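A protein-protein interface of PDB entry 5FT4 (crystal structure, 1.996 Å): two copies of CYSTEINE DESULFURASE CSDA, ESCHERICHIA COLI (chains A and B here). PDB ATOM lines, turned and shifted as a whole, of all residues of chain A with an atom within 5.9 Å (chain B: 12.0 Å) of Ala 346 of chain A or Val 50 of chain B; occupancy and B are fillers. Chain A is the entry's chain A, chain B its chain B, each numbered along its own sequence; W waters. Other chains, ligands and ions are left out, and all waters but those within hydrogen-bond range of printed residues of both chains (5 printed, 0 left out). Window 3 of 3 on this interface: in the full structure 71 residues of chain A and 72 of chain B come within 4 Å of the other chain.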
ATOM      1  N   ASP A  18     -12.808 -20.275  -4.315  1.00  0.00           N
ATOM      2  CA  ASP A  18     -13.253 -18.889  -4.320  1.00  0.00           C
ATOM      3  C   ASP A  18     -14.774 -18.721  -4.369  1.00  0.00           C
ATOM      4  O   ASP A  18     -15.304 -17.706  -3.903  1.00  0.00           O
ATOM      5  CB  ASP A  18     -12.617 -18.159  -5.491  1.00  0.00           C
ATOM      6  CG  ASP A  18     -13.242 -16.793  -5.733  1.00  0.00           C
ATOM      7  OD1 ASP A  18     -13.030 -15.874  -4.896  1.00  0.00           O
ATOM      8  OD2 ASP A  18     -13.936 -16.655  -6.783  1.00  0.00           O
ATOM      9  N   ALA A  19     -15.462 -19.700  -4.952  1.00  0.00           N
ATOM     10  CA  ALA A  19     -16.914 -19.628  -5.202  1.00  0.00           C
ATOM     11  C   ALA A  19     -17.840 -19.595  -3.966  1.00  0.00           C
ATOM     12  O   ALA A  19     -18.990 -19.186  -4.064  1.00  0.00           O
ATOM     13  CB  ALA A  19     -17.330 -20.795  -6.080  1.00  0.00           C
ATOM     14  N   GLY A  20     -17.325 -19.962  -2.814  1.00  0.00           N
ATOM     15  CA  GLY A  20     -18.138 -20.087  -1.621  1.00  0.00           C
ATOM     16  C   GLY A  20     -19.049 -21.289  -1.747  1.00  0.00           C
ATOM     17  O   GLY A  20     -18.662 -22.337  -2.295  1.00  0.00           O
ATOM     18  N   VAL A  21     -20.277 -21.129  -1.267  1.00  0.00           N
ATOM     19  CA  VAL A  21     -21.268 -22.180  -1.360  1.00  0.00           C
ATOM     20  C   VAL A  21     -22.046 -21.919  -2.651  1.00  0.00           C
ATOM     21  O   VAL A  21     -22.897 -21.008  -2.717  1.00  0.00           O
ATOM     22  CB  VAL A  21     -22.186 -22.199  -0.133  1.00  0.00           C
ATOM     23  CG1 VAL A  21     -23.211 -23.317  -0.248  1.00  0.00           C
ATOM     24  CG2 VAL A  21     -21.371 -22.377   1.097  1.00  0.00           C
ATOM     25  N   MET A 341     -33.301 -11.300   0.203  1.00  0.00           N
ATOM     26  CA  MET A 341     -32.788 -12.572   0.673  1.00  0.00           C
ATOM     27  C   MET A 341     -31.594 -13.054  -0.154  1.00  0.00           C
ATOM     28  O   MET A 341     -30.608 -13.557   0.399  1.00  0.00           O
ATOM     29  CB  MET A 341     -33.900 -13.616   0.670  1.00  0.00           C
ATOM     30  CG  MET A 341     -33.457 -14.913   1.298  1.00  0.00           C
ATOM     31  SD  MET A 341     -34.787 -15.898   1.978  1.00  0.00           S
ATOM     32  CE  MET A 341     -34.742 -15.295   3.653  1.00  0.00           C
ATOM     33  N   VAL A 342     -31.669 -12.892  -1.474  1.00  0.00           N
ATOM     34  CA  VAL A 342     -30.548 -13.248  -2.357  1.00  0.00           C
ATOM     35  C   VAL A 342     -29.266 -12.475  -1.978  1.00  0.00           C
ATOM     36  O   VAL A 342     -28.175 -13.052  -1.885  1.00  0.00           O
ATOM     37  CB  VAL A 342     -30.903 -12.985  -3.857  1.00  0.00           C
ATOM     38  CG1 VAL A 342     -29.672 -13.044  -4.729  1.00  0.00           C
ATOM     39  CG2 VAL A 342     -31.994 -13.976  -4.331  1.00  0.00           C
ATOM     40  N   THR A 343     -29.406 -11.167  -1.784  1.00  0.00           N
ATOM     41  CA  THR A 343     -28.284 -10.294  -1.396  1.00  0.00           C
ATOM     42  C   THR A 343     -27.644 -10.692  -0.059  1.00  0.00           C
ATOM     43  O   THR A 343     -26.419 -10.839   0.049  1.00  0.00           O
ATOM     44  CB  THR A 343     -28.748  -8.836  -1.290  1.00  0.00           C
ATOM     45  OG1 THR A 343     -29.145  -8.379  -2.584  1.00  0.00           O
ATOM     46  CG2 THR A 343     -27.643  -7.943  -0.739  1.00  0.00           C
ATOM     47  N   LEU A 344     -28.464 -10.864   0.962  1.00  0.00           N
ATOM     48  CA  LEU A 344     -27.947 -11.273   2.256  1.00  0.00           C
ATOM     49  C   LEU A 344     -27.286 -12.642   2.166  1.00  0.00           C
ATOM     50  O   LEU A 344     -26.202 -12.847   2.734  1.00  0.00           O
ATOM     51  CB  LEU A 344     -29.073 -11.281   3.297  1.00  0.00           C
ATOM     52  CG  LEU A 344     -29.567  -9.920   3.760  1.00  0.00           C
ATOM     53  CD1 LEU A 344     -30.822 -10.041   4.602  1.00  0.00           C
ATOM     54  CD2 LEU A 344     -28.486  -9.258   4.594  1.00  0.00           C
ATOM     55  N   LEU A 345     -27.881 -13.553   1.394  1.00  0.00           N
ATOM     56  CA  LEU A 345     -27.325 -14.896   1.287  1.00  0.00           C
ATOM     57  C   LEU A 345     -25.932 -14.810   0.647  1.00  0.00           C
ATOM     58  O   LEU A 345     -25.005 -15.468   1.097  1.00  0.00           O
ATOM     59  CB  LEU A 345     -28.232 -15.829   0.445  1.00  0.00           C
ATOM     60  CG  LEU A 345     -29.484 -16.456   1.087  1.00  0.00           C
ATOM     61  CD1 LEU A 345     -29.942 -17.732   0.413  1.00  0.00           C
ATOM     62  CD2 LEU A 345     -29.340 -16.650   2.515  1.00  0.00           C
ATOM     63  N   ALA A 346     -25.791 -13.967  -0.378  1.00  0.00           N
ATOM     64  CA  ALA A 346     -24.494 -13.820  -1.042  1.00  0.00           C
ATOM     65  C   ALA A 346     -23.465 -13.227  -0.082  1.00  0.00           C
ATOM     66  O   ALA A 346     -22.328 -13.687  -0.023  1.00  0.00           O
ATOM     67  CB  ALA A 346     -24.615 -12.957  -2.298  1.00  0.00           C
ATOM     68  N   GLU A 347     -23.867 -12.217   0.672  1.00  0.00           N
ATOM     69  CA  GLU A 347     -22.975 -11.635   1.656  1.00  0.00           C
ATOM     70  C   GLU A 347     -22.554 -12.635   2.715  1.00  0.00           C
ATOM     71  O   GLU A 347     -21.410 -12.586   3.158  1.00  0.00           O
ATOM     72  CB  GLU A 347     -23.612 -10.404   2.294  1.00  0.00           C
ATOM     73  CG  GLU A 347     -23.864  -9.300   1.255  1.00  0.00           C
ATOM     74  CD  GLU A 347     -24.628  -8.105   1.815  1.00  0.00           C
ATOM     75  OE1 GLU A 347     -25.447  -8.294   2.737  1.00  0.00           O
ATOM     76  OE2 GLU A 347     -24.426  -6.979   1.310  1.00  0.00           O
ATOM     77  N   TYR A 348     -23.441 -13.569   3.064  1.00  0.00           N
ATOM     78  CA  TYR A 348     -23.082 -14.652   3.996  1.00  0.00           C
ATOM     79  C   TYR A 348     -22.391 -15.828   3.220  1.00  0.00           C
ATOM     80  O   TYR A 348     -22.046 -16.849   3.796  1.00  0.00           O
ATOM     81  CB  TYR A 348     -24.320 -15.146   4.781  1.00  0.00           C
ATOM     82  CG  TYR A 348     -24.663 -14.278   5.978  1.00  0.00           C
ATOM     83  CD1 TYR A 348     -23.834 -14.218   7.079  1.00  0.00           C
ATOM     84  CD2 TYR A 348     -25.830 -13.533   6.014  1.00  0.00           C
ATOM     85  CE1 TYR A 348     -24.151 -13.424   8.188  1.00  0.00           C
ATOM     86  CE2 TYR A 348     -26.149 -12.719   7.111  1.00  0.00           C
ATOM     87  CZ  TYR A 348     -25.306 -12.676   8.193  1.00  0.00           C
ATOM     88  OH  TYR A 348     -25.616 -11.889   9.286  1.00  0.00           O
ATOM     89  N   GLY A 349     -22.148 -15.642   1.921  1.00  0.00           N
ATOM     90  CA  GLY A 349     -21.350 -16.580   1.134  1.00  0.00           C
ATOM     91  C   GLY A 349     -22.056 -17.694   0.380  1.00  0.00           C
ATOM     92  O   GLY A 349     -21.405 -18.665  -0.048  1.00  0.00           O
ATOM     93  N   ILE A 350     -23.367 -17.528   0.181  1.00  0.00           N
ATOM     94  CA  ILE A 350     -24.190 -18.478  -0.552  1.00  0.00           C
ATOM     95  C   ILE A 350     -24.592 -17.885  -1.906  1.00  0.00           C
ATOM     96  O   ILE A 350     -25.269 -16.849  -1.963  1.00  0.00           O
ATOM     97  CB  ILE A 350     -25.503 -18.839   0.168  1.00  0.00           C
ATOM     98  CG1 ILE A 350     -25.291 -18.992   1.681  1.00  0.00           C
ATOM     99  CG2 ILE A 350     -26.139 -20.047  -0.516  1.00  0.00           C
ATOM    100  CD1 ILE A 350     -24.261 -19.999   2.066  1.00  0.00           C
ATOM    101  N   ALA A 351     -24.214 -18.578  -2.967  1.00  0.00           N
ATOM    102  CA  ALA A 351     -24.465 -18.127  -4.328  1.00  0.00           C
ATOM    103  C   ALA A 351     -25.672 -18.850  -4.907  1.00  0.00           C
ATOM    104  O   ALA A 351     -25.610 -20.040  -5.196  1.00  0.00           O
ATOM    105  CB  ALA A 351     -23.287 -18.369  -5.157  1.00  0.00           C
ATOM    106  N   GLN B  41      -9.147 -17.470 -17.251  1.00  0.00           N
ATOM    107  CA  GLN B  41      -9.675 -16.870 -16.043  1.00  0.00           C
ATOM    108  C   GLN B  41     -11.180 -17.056 -15.983  1.00  0.00           C
ATOM    109  O   GLN B  41     -11.692 -17.470 -14.958  1.00  0.00           O
ATOM    110  CB  GLN B  41      -9.309 -15.385 -15.985  1.00  0.00           C
ATOM    111  CG  GLN B  41      -7.840 -15.160 -15.713  1.00  0.00           C
ATOM    112  CD  GLN B  41      -7.460 -13.699 -15.655  1.00  0.00           C
ATOM    113  OE1 GLN B  41      -8.305 -12.830 -15.441  1.00  0.00           O
ATOM    114  NE2 GLN B  41      -6.181 -13.415 -15.893  1.00  0.00           N
ATOM    115  N   PHE B  42     -11.880 -16.817 -17.094  1.00  0.00           N
ATOM    116  CA  PHE B  42     -13.335 -16.908 -17.109  1.00  0.00           C
ATOM    117  C   PHE B  42     -13.845 -18.303 -16.780  1.00  0.00           C
ATOM    118  O   PHE B  42     -14.855 -18.466 -16.084  1.00  0.00           O
ATOM    119  CB  PHE B  42     -13.902 -16.489 -18.488  1.00  0.00           C
ATOM    120  CG  PHE B  42     -15.384 -16.773 -18.643  1.00  0.00           C
ATOM    121  CD1 PHE B  42     -16.317 -16.036 -17.937  1.00  0.00           C
ATOM    122  CD2 PHE B  42     -15.832 -17.810 -19.463  1.00  0.00           C
ATOM    123  CE1 PHE B  42     -17.678 -16.321 -18.032  1.00  0.00           C
ATOM    124  CE2 PHE B  42     -17.169 -18.104 -19.582  1.00  0.00           C
ATOM    125  CZ  PHE B  42     -18.116 -17.358 -18.858  1.00  0.00           C
ATOM    126  N   SER B  44     -12.249 -20.469 -14.985  1.00  0.00           N
ATOM    127  CA  SER B  44     -11.623 -20.922 -13.740  1.00  0.00           C
ATOM    128  C   SER B  44     -12.190 -20.233 -12.498  1.00  0.00           C
ATOM    129  O   SER B  44     -11.796 -20.548 -11.389  1.00  0.00           O
ATOM    130  CB  SER B  44     -10.106 -20.695 -13.793  1.00  0.00           C
ATOM    131  OG  SER B  44      -9.529 -21.357 -14.902  1.00  0.00           O
ATOM    132  N   LEU B  45     -13.133 -19.319 -12.706  1.00  0.00           N
ATOM    133  CA  LEU B  45     -13.824 -18.602 -11.622  1.00  0.00           C
ATOM    134  C   LEU B  45     -15.342 -18.727 -11.722  1.00  0.00           C
ATOM    135  O   LEU B  45     -15.912 -18.782 -12.831  1.00  0.00           O
ATOM    136  CB  LEU B  45     -13.502 -17.104 -11.634  1.00  0.00           C
ATOM    137  CG  LEU B  45     -12.174 -16.550 -11.148  1.00  0.00           C
ATOM    138  CD1 LEU B  45     -12.316 -15.040 -11.050  1.00  0.00           C
ATOM    139  CD2 LEU B  45     -11.715 -17.189  -9.838  1.00  0.00           C
ATOM    140  N   SER B  46     -16.009 -18.683 -10.572  1.00  0.00           N
ATOM    141  CA  SER B  46     -17.469 -18.590 -10.543  1.00  0.00           C
ATOM    142  C   SER B  46     -17.978 -17.353 -11.280  1.00  0.00           C
ATOM    143  O   SER B  46     -17.381 -16.289 -11.167  1.00  0.00           O
ATOM    144  CB  SER B  46     -17.968 -18.529  -9.096  1.00  0.00           C
ATOM    145  OG  SER B  46     -19.374 -18.353  -9.054  1.00  0.00           O
ATOM    146  N   ALA B  47     -19.086 -17.497 -12.005  1.00  0.00           N
ATOM    147  CA  ALA B  47     -19.833 -16.351 -12.559  1.00  0.00           C
ATOM    148  C   ALA B  47     -21.008 -15.966 -11.640  1.00  0.00           C
ATOM    149  O   ALA B  47     -21.783 -15.036 -11.919  1.00  0.00           O
ATOM    150  CB  ALA B  47     -20.325 -16.656 -13.952  1.00  0.00           C
ATOM    151  N   GLY B  48     -21.089 -16.614 -10.492  1.00  0.00           N
ATOM    152  CA  GLY B  48     -22.110 -16.273  -9.497  1.00  0.00           C
ATOM    153  C   GLY B  48     -21.800 -15.009  -8.704  1.00  0.00           C
ATOM    154  O   GLY B  48     -20.822 -14.282  -9.006  1.00  0.00           O
ATOM    155  N   ASN B  49     -22.618 -14.759  -7.673  1.00  0.00           N
ATOM    156  CA  ASN B  49     -22.554 -13.509  -6.926  1.00  0.00           C
ATOM    157  C   ASN B  49     -21.662 -13.555  -5.694  1.00  0.00           C
ATOM    158  O   ASN B  49     -21.657 -12.609  -4.911  1.00  0.00           O
ATOM    159  CB  ASN B  49     -23.972 -13.044  -6.532  1.00  0.00           C
ATOM    160  CG  ASN B  49     -24.803 -14.114  -5.803  1.00  0.00           C
ATOM    161  OD1 ASN B  49     -24.326 -15.180  -5.462  1.00  0.00           O
ATOM    162  ND2 ASN B  49     -26.073 -13.808  -5.579  1.00  0.00           N
ATOM    163  N   VAL B  50     -20.964 -14.671  -5.486  1.00  0.00           N
ATOM    164  CA  VAL B  50     -20.042 -14.803  -4.350  1.00  0.00           C
ATOM    165  C   VAL B  50     -18.575 -14.953  -4.842  1.00  0.00           C
ATOM    166  O   VAL B  50     -18.281 -15.664  -5.810  1.00  0.00           O
ATOM    167  CB  VAL B  50     -20.432 -15.989  -3.440  1.00  0.00           C
ATOM    168  CG1 VAL B  50     -19.382 -16.227  -2.363  1.00  0.00           C
ATOM    169  CG2 VAL B  50     -21.795 -15.718  -2.721  1.00  0.00           C
ATOM    170  N   HIS B  51     -17.682 -14.248  -4.175  1.00  0.00           N
ATOM    171  CA  HIS B  51     -16.239 -14.360  -4.365  1.00  0.00           C
ATOM    172  C   HIS B  51     -15.547 -14.176  -3.046  1.00  0.00           C
ATOM    173  O   HIS B  51     -15.610 -13.107  -2.427  1.00  0.00           O
ATOM    174  CB  HIS B  51     -15.720 -13.357  -5.374  1.00  0.00           C
ATOM    175  CG  HIS B  51     -16.173 -13.654  -6.758  1.00  0.00           C
ATOM    176  ND1 HIS B  51     -15.666 -14.709  -7.492  1.00  0.00           N
ATOM    177  CD2 HIS B  51     -17.146 -13.097  -7.510  1.00  0.00           C
ATOM    178  CE1 HIS B  51     -16.283 -14.754  -8.661  1.00  0.00           C
ATOM    179  NE2 HIS B  51     -17.182 -13.785  -8.699  1.00  0.00           N
ATOM    180  N   ARG B  52     -14.943 -15.232  -2.557  1.00  0.00           N
ATOM    181  CA  ARG B  52     -14.345 -15.126  -1.249  1.00  0.00           C
ATOM    182  C   ARG B  52     -13.075 -14.277  -1.270  1.00  0.00           C
ATOM    183  O   ARG B  52     -12.740 -13.664  -0.255  1.00  0.00           O
ATOM    184  CB  ARG B  52     -14.028 -16.502  -0.709  1.00  0.00           C
ATOM    185  CG  ARG B  52     -15.214 -17.307  -0.212  1.00  0.00           C
ATOM    186  CD  ARG B  52     -14.689 -18.540   0.519  1.00  0.00           C
ATOM    187  NE  ARG B  52     -15.715 -19.460   1.013  1.00  0.00           N
ATOM    188  CZ  ARG B  52     -15.742 -20.775   0.776  1.00  0.00           C
ATOM    189  NH1 ARG B  52     -14.814 -21.360   0.021  1.00  0.00           N
ATOM    190  NH2 ARG B  52     -16.722 -21.515   1.283  1.00  0.00           N
ATOM    191  N   SER B  53     -12.361 -14.252  -2.397  1.00  0.00           N
ATOM    192  CA  SER B  53     -11.072 -13.584  -2.472  1.00  0.00           C
ATOM    193  C   SER B  53     -10.664 -13.101  -3.864  1.00  0.00           C
ATOM    194  O   SER B  53      -9.685 -12.366  -3.962  1.00  0.00           O
ATOM    195  CB  SER B  53      -9.942 -14.498  -1.982  1.00  0.00           C
ATOM    196  OG  SER B  53      -9.564 -15.430  -2.988  1.00  0.00           O
ATOM    197  N   GLN B  54     -11.359 -13.505  -4.932  1.00  0.00           N
ATOM    198  CA  GLN B  54     -10.917 -13.126  -6.282  1.00  0.00           C
ATOM    199  C   GLN B  54     -11.842 -12.080  -6.884  1.00  0.00           C
ATOM    200  O   GLN B  54     -12.008 -12.002  -8.113  1.00  0.00           O
ATOM    201  CB  GLN B  54     -10.843 -14.342  -7.227  1.00  0.00           C
ATOM    202  CG  GLN B  54      -9.904 -15.461  -6.791  1.00  0.00           C
ATOM    203  CD  GLN B  54      -8.447 -15.029  -6.779  1.00  0.00           C
ATOM    204  OE1 GLN B  54      -7.932 -14.515  -7.773  1.00  0.00           O
ATOM    205  NE2 GLN B  54      -7.776 -15.234  -5.646  1.00  0.00           N
ATOM    206  N   PHE B  55     -12.363 -11.215  -6.026  1.00  0.00           N
ATOM    207  CA  PHE B  55     -13.250 -10.145  -6.467  1.00  0.00           C
ATOM    208  C   PHE B  55     -12.599  -9.289  -7.551  1.00  0.00           C
ATOM    209  O   PHE B  55     -13.244  -8.999  -8.555  1.00  0.00           O
ATOM    210  CB  PHE B  55     -13.691  -9.287  -5.273  1.00  0.00           C
ATOM    211  CG  PHE B  55     -14.752  -8.269  -5.617  1.00  0.00           C
ATOM    212  CD1 PHE B  55     -16.070  -8.660  -5.803  1.00  0.00           C
ATOM    213  CD2 PHE B  55     -14.441  -6.917  -5.712  1.00  0.00           C
ATOM    214  CE1 PHE B  55     -17.049  -7.730  -6.114  1.00  0.00           C
ATOM    215  CE2 PHE B  55     -15.421  -5.983  -6.015  1.00  0.00           C
ATOM    216  CZ  PHE B  55     -16.726  -6.391  -6.210  1.00  0.00           C
ATOM    217  N   ALA B  56     -11.335  -8.922  -7.389  1.00  0.00           N
ATOM    218  CA  ALA B  56     -10.647  -8.096  -8.392  1.00  0.00           C
ATOM    219  C   ALA B  56     -10.601  -8.755  -9.789  1.00  0.00           C
ATOM    220  O   ALA B  56     -10.845  -8.100 -10.801  1.00  0.00           O
ATOM    221  CB  ALA B  56      -9.209  -7.767  -7.914  1.00  0.00           C
ATOM    222  N   GLU B  57     -10.279 -10.043  -9.832  1.00  0.00           N
ATOM    223  CA  GLU B  57     -10.232 -10.798 -11.080  1.00  0.00           C
ATOM    224  C   GLU B  57     -11.649 -10.944 -11.641  1.00  0.00           C
ATOM    225  O   GLU B  57     -11.874 -10.826 -12.854  1.00  0.00           O
ATOM    226  CB  GLU B  57      -9.616 -12.181 -10.858  1.00  0.00           C
ATOM    227  CG  GLU B  57      -9.697 -13.120 -12.057  1.00  0.00           C
ATOM    228  CD  GLU B  57      -9.050 -14.480 -11.794  1.00  0.00           C
ATOM    229  OE1 GLU B  57      -8.424 -14.652 -10.725  1.00  0.00           O
ATOM    230  OE2 GLU B  57      -9.164 -15.378 -12.658  1.00  0.00           O
ATOM    231  N   ALA B  58     -12.615 -11.183 -10.762  1.00  0.00           N
ATOM    232  CA  ALA B  58     -14.009 -11.261 -11.227  1.00  0.00           C
ATOM    233  C   ALA B  58     -14.492  -9.915 -11.803  1.00  0.00           C
ATOM    234  O   ALA B  58     -15.135  -9.882 -12.854  1.00  0.00           O
ATOM    235  CB  ALA B  58     -14.930 -11.726 -10.092  1.00  0.00           C
ATOM    236  N   GLN B  59     -14.181  -8.822 -11.114  1.00  0.00           N
ATOM    237  CA  GLN B  59     -14.578  -7.503 -11.553  1.00  0.00           C
ATOM    238  C   GLN B  59     -13.959  -7.153 -12.920  1.00  0.00           C
ATOM    239  O   GLN B  59     -14.580  -6.474 -13.733  1.00  0.00           O
ATOM    240  CB  GLN B  59     -14.176  -6.456 -10.511  1.00  0.00           C
ATOM    241  CG  GLN B  59     -15.039  -6.453  -9.267  1.00  0.00           C
ATOM    242  CD  GLN B  59     -16.356  -5.729  -9.462  1.00  0.00           C
ATOM    243  OE1 GLN B  59     -17.210  -6.161 -10.242  1.00  0.00           O
ATOM    244  NE2 GLN B  59     -16.527  -4.613  -8.749  1.00  0.00           N
ATOM    245  N   LEU B  61     -13.130  -9.347 -15.328  1.00  0.00           N
ATOM    246  CA  LEU B  61     -13.902 -10.116 -16.313  1.00  0.00           C
ATOM    247  C   LEU B  61     -15.224  -9.432 -16.606  1.00  0.00           C
ATOM    248  O   LEU B  61     -15.613  -9.295 -17.746  1.00  0.00           O
ATOM    249  CB  LEU B  61     -14.159 -11.535 -15.818  1.00  0.00           C
ATOM    250  CG  LEU B  61     -12.947 -12.474 -15.729  1.00  0.00           C
ATOM    251  CD1 LEU B  61     -13.325 -13.777 -15.004  1.00  0.00           C
ATOM    252  CD2 LEU B  61     -12.430 -12.769 -17.132  1.00  0.00           C
ATOM    253  N   THR B  62     -15.914  -8.988 -15.569  1.00  0.00           N
ATOM    254  CA  THR B  62     -17.177  -8.307 -15.773  1.00  0.00           C
ATOM    255  C   THR B  62     -16.926  -7.029 -16.579  1.00  0.00           C
ATOM    256  O   THR B  62     -17.679  -6.732 -17.484  1.00  0.00           O
ATOM    257  CB  THR B  62     -17.867  -7.997 -14.435  1.00  0.00           C
ATOM    258  OG1 THR B  62     -18.204  -9.242 -13.792  1.00  0.00           O
ATOM    259  CG2 THR B  62     -19.127  -7.158 -14.640  1.00  0.00           C
HETATM  260  O   HOH W   1     -16.054 -23.906  -1.775  1.00  0.00           O
HETATM  261  O   HOH W   2     -14.572 -18.993  -8.039  1.00  0.00           O
HETATM  262  O   HOH W   3     -20.018 -17.620  -6.588  1.00  0.00           O
HETATM  263  O   HOH W   4     -27.193 -15.423  -3.304  1.00  0.00           O
HETATM  264  O   HOH W   5     -18.738 -19.445   1.457  1.00  0.00           O
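The backbone carbonyl oxygen of Asp 18 of chain A sits at hydrogen-bond distance from the backbone NH of Arg 52 of chain B, 2.8 Å away. OD1 of Asp 18 of chain A sits at hydrogen-bond distance from N of Gln 54 of chain B (2.9 Å). OD2 of Asp 18 of chain A is in hydrogen-bond range of ND1 of His 51 of chain B (2.7 Å). The backbone NH of Ser 53 of chain B sits at hydrogen-bond distance from the side-chain carboxylate of Asp 18 of chain A.
OE1 of Glu 57 of chain B sits close to OE1 of Gln 54 of chain B (3.0 Å). The backbone carbonyl oxygen (O) of Leu 345 of chain A lies within hydrogen-bond range of the backbone NH (N) of Ile 350 of chain A (2.8 Å). The backbone carbonyl oxygen (O) of Val 21 of chain A sits at hydrogen-bond distance from the backbone NH (N) of Ala 351 of chain A, 2.8 Å away. The backbone NH of Gly 48 of chain B lies within hydrogen-bond range of the side-chain hydroxyl of Ser 46 of chain B, at 2.8 Å. N of Val 21 of chain A is in hydrogen-bond range of O of Gly 349 of chain A, 3.0 Å away. The side-chain amide nitrogen (NE2) of Gln 54 of chain B sits at hydrogen-bond distance from the side-chain hydroxyl (OG) of Ser 53 of chain B, at 3.2 Å.
Among the printed residues, pairs that only touch across the chains: Asp 18 of chain A with Leu 45 of chain B (3.8 Å), Ala 19 of chain A with Ser 46 of chain B (3.8 Å), Ala 19 of chain A with Val 50 of chain B (3.4 Å), Gly 20 of chain A with Arg 52 of chain B (3.5 Å), Val 342 of chain A with Asn 49 of chain B (3.8 Å), Ala 346 of chain A with Asn 49 of chain B (3.7 Å), Ala 346 of chain A with Val 50 of chain B (3.4 Å), Gly 349 of chain A with Val 50 of chain B (3.7 Å), Ile 350 of chain A with Asn 49 of chain B (3.99 Å), Ile 350 of chain A with Val 50 of chain B (3.6 Å), Ala 351 of chain A with Asn 49 of chain B (3.2 Å) and Ala 351 of chain A with Val 50 of chain B (3.8 Å).
Ala 346 of chain A touches two residues of chain B. Printed residues of chain A within 4 Å of Val 50 of chain B: Ala 19 (3.4 Å), Ala 346 (3.4 Å), Gly 349 (3.7 Å), Ile 350 (3.6 Å) and Ala 351 (3.8 Å). Of chain B, only Leu 45, His 51, Arg 52, Ser 53 and Gln 54 come within 4 Å of Asp 18 of chain A. Ala 19 of chain A touches just these residues of chain B: Ser 46 (3.8 Å) and Val 50 (3.4 Å). Gly 20 of chain A touches one residue of chain B. No residue of chain B comes within 4 Å of Thr 343 of chain A. No residue of chain B comes within 4 Å of Leu 345 of chain A. No residue of chain B comes within 4 Å of Glu 347 of chain A. Of the printed residues of chain B, Gly 349 of chain A touches Val 50. Of chain B, only Asn 49 (3.2 Å) and Val 50 (3.8 Å) come within 4 Å of Ala 351 of chain A. Of the printed residues of chain A, Leu 45 of chain B touches Asp 18 (3.8 Å). Of the printed residues of chain A, His 51 of chain B touches Asp 18. Printed residues of chain A within 4 Å of Ser 53 of chain B: Asp 18. The nearest residue of chain B that does not touch Ala 346 of chain A is His 51 of chain B (6.3 Å). The nearest printed residue of chain A that does not touch Ser 46 of chain B is Asp 18 of chain A (4.8 Å).
Of the 20 printed residues of chain B, 8 touch a printed residue of chain A. Hydrophobic or aromatic side chains of chain B within 4 Å of the printed part of chain A: Leu 45, Val 50 and His 51. Hydrophobic or aromatic side chains of chain A that line the printed part of chain B: Ala 19, Val 342, Ala 346 and Ala 351.
No position is printed for both chains. Of the 16 pairs that touch across the chains among the printed residues, none has its exchanged pair printed and touching as well.
Water W3 lies within hydrogen-bond range of OG of Ser 46 of chain B (2.7 Å), O of Val 50 of chain B (2.7 Å) and O of Ala 19 of chain A (3.1 Å). Water W2 lies within hydrogen-bond range of OD2 of Asp 18 of chain A, N of Ser 46 of chain B and N of Ala 19 of chain A. Water W4 lies within hydrogen-bond range of the backbone carbonyl oxygen (O) of Ile 350 of chain A (2.7 Å), the backbone carbonyl oxygen (O) of Val 342 of chain A (2.9 Å) and the side-chain amide nitrogen (ND2) of Asn 49 of chain B (3.0 Å). Water W5 bridges the guanidinium group of Arg 52 of chain B (2.9 Å) and the backbone carbonyl oxygen of Gly 349 of chain A (3.2 Å). Water W1 bridges the backbone carbonyl oxygen (O) of Gly 20 of chain A and the guanidinium group (NH1) of Arg 52 of chain B.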
